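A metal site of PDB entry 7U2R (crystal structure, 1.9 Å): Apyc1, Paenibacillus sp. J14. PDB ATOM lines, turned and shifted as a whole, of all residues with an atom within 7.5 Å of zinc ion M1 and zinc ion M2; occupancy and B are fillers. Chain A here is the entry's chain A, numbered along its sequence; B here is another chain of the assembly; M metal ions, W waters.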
ATOM      1  N   GLY A  11      31.354   9.803 -25.914  1.00  0.00           N
ATOM      2  CA  GLY A  11      32.194   9.904 -27.090  1.00  0.00           C
ATOM      3  C   GLY A  11      31.932  11.146 -27.932  1.00  0.00           C
ATOM      4  O   GLY A  11      30.881  11.753 -27.844  1.00  0.00           O
ATOM      5  N   GLY A  12      32.926  11.524 -28.721  1.00  0.00           N
ATOM      6  CA  GLY A  12      32.725  12.536 -29.740  1.00  0.00           C
ATOM      7  C   GLY A  12      31.810  11.982 -30.826  1.00  0.00           C
ATOM      8  O   GLY A  12      31.402  10.812 -30.802  1.00  0.00           O
ATOM      9  N   ALA A  13      31.521  12.828 -31.817  1.00  0.00           N
ATOM     10  CA  ALA A  13      30.467  12.508 -32.793  1.00  0.00           C
ATOM     11  C   ALA A  13      30.729  11.209 -33.548  1.00  0.00           C
ATOM     12  O   ALA A  13      29.783  10.500 -33.912  1.00  0.00           O
ATOM     13  CB  ALA A  13      30.322  13.652 -33.815  1.00  0.00           C
ATOM     14  N   ASN A  20      27.226   8.394 -28.266  1.00  0.00           N
ATOM     15  CA  ASN A  20      27.174   9.849 -28.381  1.00  0.00           C
ATOM     16  C   ASN A  20      27.115  10.486 -26.985  1.00  0.00           C
ATOM     17  O   ASN A  20      26.584   9.900 -26.042  1.00  0.00           O
ATOM     18  CB  ASN A  20      25.917  10.338 -29.135  1.00  0.00           C
ATOM     19  CG  ASN A  20      25.819   9.909 -30.575  1.00  0.00           C
ATOM     20  OD1 ASN A  20      24.713   9.948 -31.134  1.00  0.00           O
ATOM     21  ND2 ASN A  20      26.921   9.537 -31.221  1.00  0.00           N
ATOM     22  N   ASN A  21      27.604  11.708 -26.873  1.00  0.00           N
ATOM     23  CA  ASN A  21      27.793  12.360 -25.567  1.00  0.00           C
ATOM     24  C   ASN A  21      26.466  12.926 -25.071  1.00  0.00           C
ATOM     25  O   ASN A  21      26.097  14.082 -25.342  1.00  0.00           O
ATOM     26  CB  ASN A  21      28.861  13.443 -25.687  1.00  0.00           C
ATOM     27  CG  ASN A  21      29.422  13.835 -24.368  1.00  0.00           C
ATOM     28  OD1 ASN A  21      30.107  13.049 -23.736  1.00  0.00           O
ATOM     29  ND2 ASN A  21      29.133  15.066 -23.937  1.00  0.00           N
ATOM     30  N   ASN A  22      25.711  12.092 -24.364  1.00  0.00           N
ATOM     31  CA  ASN A  22      24.369  12.439 -23.926  1.00  0.00           C
ATOM     32  C   ASN A  22      24.282  12.044 -22.460  1.00  0.00           C
ATOM     33  O   ASN A  22      24.788  10.984 -22.080  1.00  0.00           O
ATOM     34  CB  ASN A  22      23.237  11.675 -24.704  1.00  0.00           C
ATOM     35  CG  ASN A  22      23.327  11.764 -26.242  1.00  0.00           C
ATOM     36  OD1 ASN A  22      22.822  10.860 -26.911  1.00  0.00           O
ATOM     37  ND2 ASN A  22      23.897  12.844 -26.798  1.00  0.00           N
ATOM     38  N   ASP A  35      20.515  15.968 -24.347  1.00  0.00           N
ATOM     39  CA  ASP A  35      20.827  15.551 -25.706  1.00  0.00           C
ATOM     40  C   ASP A  35      20.464  14.094 -25.970  1.00  0.00           C
ATOM     41  O   ASP A  35      20.371  13.268 -25.054  1.00  0.00           O
ATOM     42  CB  ASP A  35      22.290  15.852 -26.054  1.00  0.00           C
ATOM     43  CG  ASP A  35      22.542  17.371 -26.135  1.00  0.00           C
ATOM     44  OD1 ASP A  35      21.547  18.092 -26.419  1.00  0.00           O
ATOM     45  OD2 ASP A  35      23.698  17.847 -25.995  1.00  0.00           O
ATOM     46  N   THR A  60      20.959  20.986 -26.454  1.00  0.00           N
ATOM     47  CA  THR A  60      21.976  22.034 -26.382  1.00  0.00           C
ATOM     48  C   THR A  60      22.285  22.673 -27.717  1.00  0.00           C
ATOM     49  O   THR A  60      22.635  23.864 -27.743  1.00  0.00           O
ATOM     50  CB  THR A  60      23.291  21.494 -25.794  1.00  0.00           C
ATOM     51  OG1 THR A  60      23.907  20.589 -26.723  1.00  0.00           O
ATOM     52  CG2 THR A  60      23.038  20.795 -24.448  1.00  0.00           C
ATOM     53  N   HIS A  61      22.183  21.934 -28.825  1.00  0.00           N
ATOM     54  CA  HIS A  61      22.416  22.455 -30.183  1.00  0.00           C
ATOM     55  C   HIS A  61      22.021  21.368 -31.177  1.00  0.00           C
ATOM     56  O   HIS A  61      21.719  20.230 -30.799  1.00  0.00           O
ATOM     57  CB  HIS A  61      23.881  22.878 -30.409  1.00  0.00           C
ATOM     58  CG  HIS A  61      24.848  21.746 -30.377  1.00  0.00           C
ATOM     59  ND1 HIS A  61      25.062  20.998 -29.241  1.00  0.00           N
ATOM     60  CD2 HIS A  61      25.652  21.213 -31.331  1.00  0.00           C
ATOM     61  CE1 HIS A  61      25.957  20.059 -29.483  1.00  0.00           C
ATOM     62  NE2 HIS A  61      26.312  20.148 -30.748  1.00  0.00           N
ATOM     63  N   ILE A  62      22.075  21.724 -32.464  1.00  0.00           N
ATOM     64  CA  ILE A  62      21.554  20.860 -33.524  1.00  0.00           C
ATOM     65  C   ILE A  62      22.717  20.190 -34.248  1.00  0.00           C
ATOM     66  O   ILE A  62      23.392  20.799 -35.082  1.00  0.00           O
ATOM     67  CB  ILE A  62      20.664  21.628 -34.498  1.00  0.00           C
ATOM     68  CG1 ILE A  62      19.486  22.217 -33.727  1.00  0.00           C
ATOM     69  CG2 ILE A  62      20.170  20.679 -35.569  1.00  0.00           C
ATOM     70  CD1 ILE A  62      18.638  23.071 -34.559  1.00  0.00           C
ATOM     71  N   HIS A  63      22.927  18.910 -33.951  1.00  0.00           N
ATOM     72  CA  HIS A  63      23.897  18.038 -34.589  1.00  0.00           C
ATOM     73  C   HIS A  63      23.396  16.632 -34.357  1.00  0.00           C
ATOM     74  O   HIS A  63      22.764  16.368 -33.329  1.00  0.00           O
ATOM     75  CB  HIS A  63      25.285  18.132 -33.968  1.00  0.00           C
ATOM     76  CG  HIS A  63      26.237  19.024 -34.675  1.00  0.00           C
ATOM     77  ND1 HIS A  63      27.325  19.553 -34.025  1.00  0.00           N
ATOM     78  CD2 HIS A  63      26.306  19.463 -35.963  1.00  0.00           C
ATOM     79  CE1 HIS A  63      27.998  20.334 -34.869  1.00  0.00           C
ATOM     80  NE2 HIS A  63      27.423  20.264 -36.054  1.00  0.00           N
ATOM     81  N   GLY A  64      23.711  15.725 -35.276  1.00  0.00           N
ATOM     82  CA  GLY A  64      23.152  14.398 -35.189  1.00  0.00           C
ATOM     83  C   GLY A  64      23.497  13.685 -33.898  1.00  0.00           C
ATOM     84  O   GLY A  64      22.695  12.871 -33.409  1.00  0.00           O
ATOM     85  N   ASP A  65      24.687  13.941 -33.345  1.00  0.00           N
ATOM     86  CA  ASP A  65      25.015  13.226 -32.109  1.00  0.00           C
ATOM     87  C   ASP A  65      24.325  13.832 -30.888  1.00  0.00           C
ATOM     88  O   ASP A  65      24.542  13.347 -29.771  1.00  0.00           O
ATOM     89  CB  ASP A  65      26.548  13.155 -31.905  1.00  0.00           C
ATOM     90  CG  ASP A  65      27.255  14.503 -32.020  1.00  0.00           C
ATOM     91  OD1 ASP A  65      26.932  15.296 -32.934  1.00  0.00           O
ATOM     92  OD2 ASP A  65      28.179  14.699 -31.224  1.00  0.00           O
ATOM     93  N   HIS A  66      23.483  14.858 -31.094  1.00  0.00           N
ATOM     94  CA  HIS A  66      22.677  15.437 -30.036  1.00  0.00           C
ATOM     95  C   HIS A  66      21.191  15.477 -30.323  1.00  0.00           C
ATOM     96  O   HIS A  66      20.414  15.641 -29.366  1.00  0.00           O
ATOM     97  CB  HIS A  66      23.159  16.889 -29.740  1.00  0.00           C
ATOM     98  CG  HIS A  66      24.613  16.913 -29.404  1.00  0.00           C
ATOM     99  ND1 HIS A  66      25.072  16.899 -28.109  1.00  0.00           N
ATOM    100  CD2 HIS A  66      25.703  16.786 -30.188  1.00  0.00           C
ATOM    101  CE1 HIS A  66      26.392  16.854 -28.110  1.00  0.00           C
ATOM    102  NE2 HIS A  66      26.789  16.791 -29.360  1.00  0.00           N
ATOM    103  N   HIS A 145      30.380  27.178 -30.814  1.00  0.00           N
ATOM    104  CA  HIS A 145      30.667  25.850 -31.349  1.00  0.00           C
ATOM    105  C   HIS A 145      30.721  25.975 -32.870  1.00  0.00           C
ATOM    106  O   HIS A 145      31.821  26.065 -33.434  1.00  0.00           O
ATOM    107  CB  HIS A 145      29.603  24.865 -30.821  1.00  0.00           C
ATOM    108  CG  HIS A 145      29.648  23.488 -31.406  1.00  0.00           C
ATOM    109  ND1 HIS A 145      30.834  22.815 -31.673  1.00  0.00           N
ATOM    110  CD2 HIS A 145      28.659  22.618 -31.718  1.00  0.00           C
ATOM    111  CE1 HIS A 145      30.566  21.614 -32.148  1.00  0.00           C
ATOM    112  NE2 HIS A 145      29.260  21.486 -32.225  1.00  0.00           N
ATOM    113  N   ILE A 146      29.596  26.012 -33.566  1.00  0.00           N
ATOM    114  CA  ILE A 146      29.577  26.229 -35.009  1.00  0.00           C
ATOM    115  C   ILE A 146      29.279  27.706 -35.265  1.00  0.00           C
ATOM    116  O   ILE A 146      28.272  28.221 -34.744  1.00  0.00           O
ATOM    117  CB  ILE A 146      28.549  25.335 -35.721  1.00  0.00           C
ATOM    118  CG1 ILE A 146      28.764  23.852 -35.370  1.00  0.00           C
ATOM    119  CG2 ILE A 146      28.702  25.543 -37.232  1.00  0.00           C
ATOM    120  CD1 ILE A 146      30.141  23.352 -35.844  1.00  0.00           C
ATOM    121  N   SER A 151      24.369  27.585 -29.926  1.00  0.00           N
ATOM    122  CA  SER A 151      24.605  26.394 -29.134  1.00  0.00           C
ATOM    123  C   SER A 151      24.784  26.830 -27.698  1.00  0.00           C
ATOM    124  O   SER A 151      25.121  27.990 -27.432  1.00  0.00           O
ATOM    125  CB  SER A 151      25.824  25.617 -29.660  1.00  0.00           C
ATOM    126  OG  SER A 151      26.995  26.399 -29.612  1.00  0.00           O
ATOM    127  N   ALA A 164      28.770  20.989 -22.662  1.00  0.00           N
ATOM    128  CA  ALA A 164      28.241  20.475 -23.932  1.00  0.00           C
ATOM    129  C   ALA A 164      29.322  20.734 -24.993  1.00  0.00           C
ATOM    130  O   ALA A 164      30.520  20.661 -24.692  1.00  0.00           O
ATOM    131  CB  ALA A 164      26.865  21.094 -24.201  1.00  0.00           C
ATOM    132  N   ASP A 165      28.963  21.002 -26.251  1.00  0.00           N
ATOM    133  CA  ASP A 165      29.966  21.183 -27.300  1.00  0.00           C
ATOM    134  C   ASP A 165      30.350  22.657 -27.343  1.00  0.00           C
ATOM    135  O   ASP A 165      29.473  23.508 -27.466  1.00  0.00           O
ATOM    136  CB  ASP A 165      29.437  20.796 -28.683  1.00  0.00           C
ATOM    137  CG  ASP A 165      29.220  19.314 -28.873  1.00  0.00           C
ATOM    138  OD1 ASP A 165      29.142  18.593 -27.858  1.00  0.00           O
ATOM    139  OD2 ASP A 165      29.053  18.966 -30.068  1.00  0.00           O
ATOM    140  N   MET A 166      31.659  22.956 -27.285  1.00  0.00           N
ATOM    141  CA  MET A 166      32.103  24.359 -27.407  1.00  0.00           C
ATOM    142  C   MET A 166      33.610  24.474 -27.626  1.00  0.00           C
ATOM    143  O   MET A 166      34.373  23.553 -27.291  1.00  0.00           O
ATOM    144  CB  MET A 166      31.715  25.178 -26.179  1.00  0.00           C
ATOM    145  CG  MET A 166      32.439  24.829 -24.888  1.00  0.00           C
ATOM    146  SD  MET A 166      31.938  26.101 -23.451  1.00  0.00           S
ATOM    147  CE  MET A 166      33.685  26.549 -22.700  1.00  0.00           C
ATOM    148  N   GLU A 188      33.924  19.041 -22.627  1.00  0.00           N
ATOM    149  CA  GLU A 188      34.259  18.310 -23.836  1.00  0.00           C
ATOM    150  C   GLU A 188      35.746  18.472 -24.159  1.00  0.00           C
ATOM    151  O   GLU A 188      36.407  19.437 -23.736  1.00  0.00           O
ATOM    152  CB  GLU A 188      33.399  18.804 -25.005  1.00  0.00           C
ATOM    153  CG  GLU A 188      33.679  20.275 -25.455  1.00  0.00           C
ATOM    154  CD  GLU A 188      34.083  20.287 -26.907  1.00  0.00           C
ATOM    155  OE1 GLU A 188      35.260  19.931 -27.223  1.00  0.00           O
ATOM    156  OE2 GLU A 188      33.211  20.592 -27.754  1.00  0.00           O
ATOM    157  N   VAL A 197      36.140  23.574 -33.837  1.00  0.00           N
ATOM    158  CA  VAL A 197      34.789  23.724 -33.319  1.00  0.00           C
ATOM    159  C   VAL A 197      34.621  23.001 -31.979  1.00  0.00           C
ATOM    160  O   VAL A 197      33.527  22.967 -31.437  1.00  0.00           O
ATOM    161  CB  VAL A 197      33.743  23.228 -34.340  1.00  0.00           C
ATOM    162  CG1 VAL A 197      33.767  24.094 -35.608  1.00  0.00           C
ATOM    163  CG2 VAL A 197      33.935  21.713 -34.635  1.00  0.00           C
ATOM    164  N   HIS A 198      35.741  22.519 -31.419  1.00  0.00           N
ATOM    165  CA  HIS A 198      35.817  21.854 -30.123  1.00  0.00           C
ATOM    166  C   HIS A 198      37.009  22.390 -29.348  1.00  0.00           C
ATOM    167  O   HIS A 198      37.851  23.131 -29.879  1.00  0.00           O
ATOM    168  CB  HIS A 198      35.939  20.317 -30.300  1.00  0.00           C
ATOM    169  CG  HIS A 198      34.700  19.704 -30.883  1.00  0.00           C
ATOM    170  ND1 HIS A 198      33.508  19.686 -30.201  1.00  0.00           N
ATOM    171  CD2 HIS A 198      34.473  19.129 -32.089  1.00  0.00           C
ATOM    172  CE1 HIS A 198      32.588  19.120 -30.948  1.00  0.00           C
ATOM    173  NE2 HIS A 198      33.136  18.760 -32.099  1.00  0.00           N
ATOM    174  N   HIS A 219      32.974  13.755 -24.386  1.00  0.00           N
ATOM    175  CA  HIS A 219      32.875  13.984 -25.829  1.00  0.00           C
ATOM    176  C   HIS A 219      34.180  13.613 -26.539  1.00  0.00           C
ATOM    177  O   HIS A 219      34.621  14.298 -27.462  1.00  0.00           O
ATOM    178  CB  HIS A 219      32.479  15.446 -26.111  1.00  0.00           C
ATOM    179  CG  HIS A 219      31.840  15.668 -27.452  1.00  0.00           C
ATOM    180  ND1 HIS A 219      32.569  15.913 -28.597  1.00  0.00           N
ATOM    181  CD2 HIS A 219      30.540  15.761 -27.803  1.00  0.00           C
ATOM    182  CE1 HIS A 219      31.741  16.094 -29.611  1.00  0.00           C
ATOM    183  NE2 HIS A 219      30.501  16.013 -29.149  1.00  0.00           N
ATOM    184  N   GLU B  71      24.164  12.281 -41.822  1.00  0.00           N
ATOM    185  CA  GLU B  71      24.969  13.397 -41.358  1.00  0.00           C
ATOM    186  C   GLU B  71      26.362  12.928 -40.978  1.00  0.00           C
ATOM    187  O   GLU B  71      27.369  13.557 -41.367  1.00  0.00           O
ATOM    188  CB  GLU B  71      24.299  14.117 -40.178  1.00  0.00           C
ATOM    189  CG  GLU B  71      25.198  15.201 -39.584  1.00  0.00           C
ATOM    190  CD  GLU B  71      24.573  15.930 -38.405  1.00  0.00           C
ATOM    191  OE1 GLU B  71      23.422  16.379 -38.507  1.00  0.00           O
ATOM    192  OE2 GLU B  71      25.233  16.040 -37.347  1.00  0.00           O
HETATM  193 ZN    ZN M   1      28.762  16.726 -30.329  1.00  0.00          ZN
HETATM  194 ZN    ZN M   2      28.032  19.666 -32.101  1.00  0.00          ZN
HETATM  195  O   HOH W   1      29.347  17.528 -32.289  1.00  0.00           O
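Zinc ion M1 is bound by water W1, NE2 of His 66, NE2 of His 219, OD2 of Asp 165 and OD2 of Asp 65. Zinc ion M1 has five donor atoms within binding distance.
The backbone carbonyl oxygen (O) of His 219 lies close to the backbone NH (N) of Gly 12 (3.5 Å). ND1 of His 145 is in hydrogen-bond range of O of Val 197 (2.7 Å). A ring nitrogen (ND1) of His 61 is in hydrogen-bond range of the side-chain hydroxyl of Thr 60 (2.8 Å). The side-chain amide oxygen (OD1) of Asn 21 sits at hydrogen-bond distance from the backbone NH (N) of His 219 (3.0 Å). A ring nitrogen (ND1) of His 66 lies within hydrogen-bond range of the side-chain carboxylate of Asp 35, 2.7 Å away. The backbone carbonyl oxygen (O) of Asp 65 is in hydrogen-bond range of the side-chain amide nitrogen (ND2) of Asn 22 (3.1 Å).
Within 4 Å of zinc ion M2: His 61, His 63, His 145 and Asp 165.
Zinc ion M2 is bound by ND1 of His 63 (2.1 Å), NE2 of His 145 (2.2 Å), NE2 of His 61 (2.2 Å), OD2 of Asp 165 (2.4 Å) and water W1 (2.5 Å). Zinc ion M2 has five donor atoms within binding distance.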
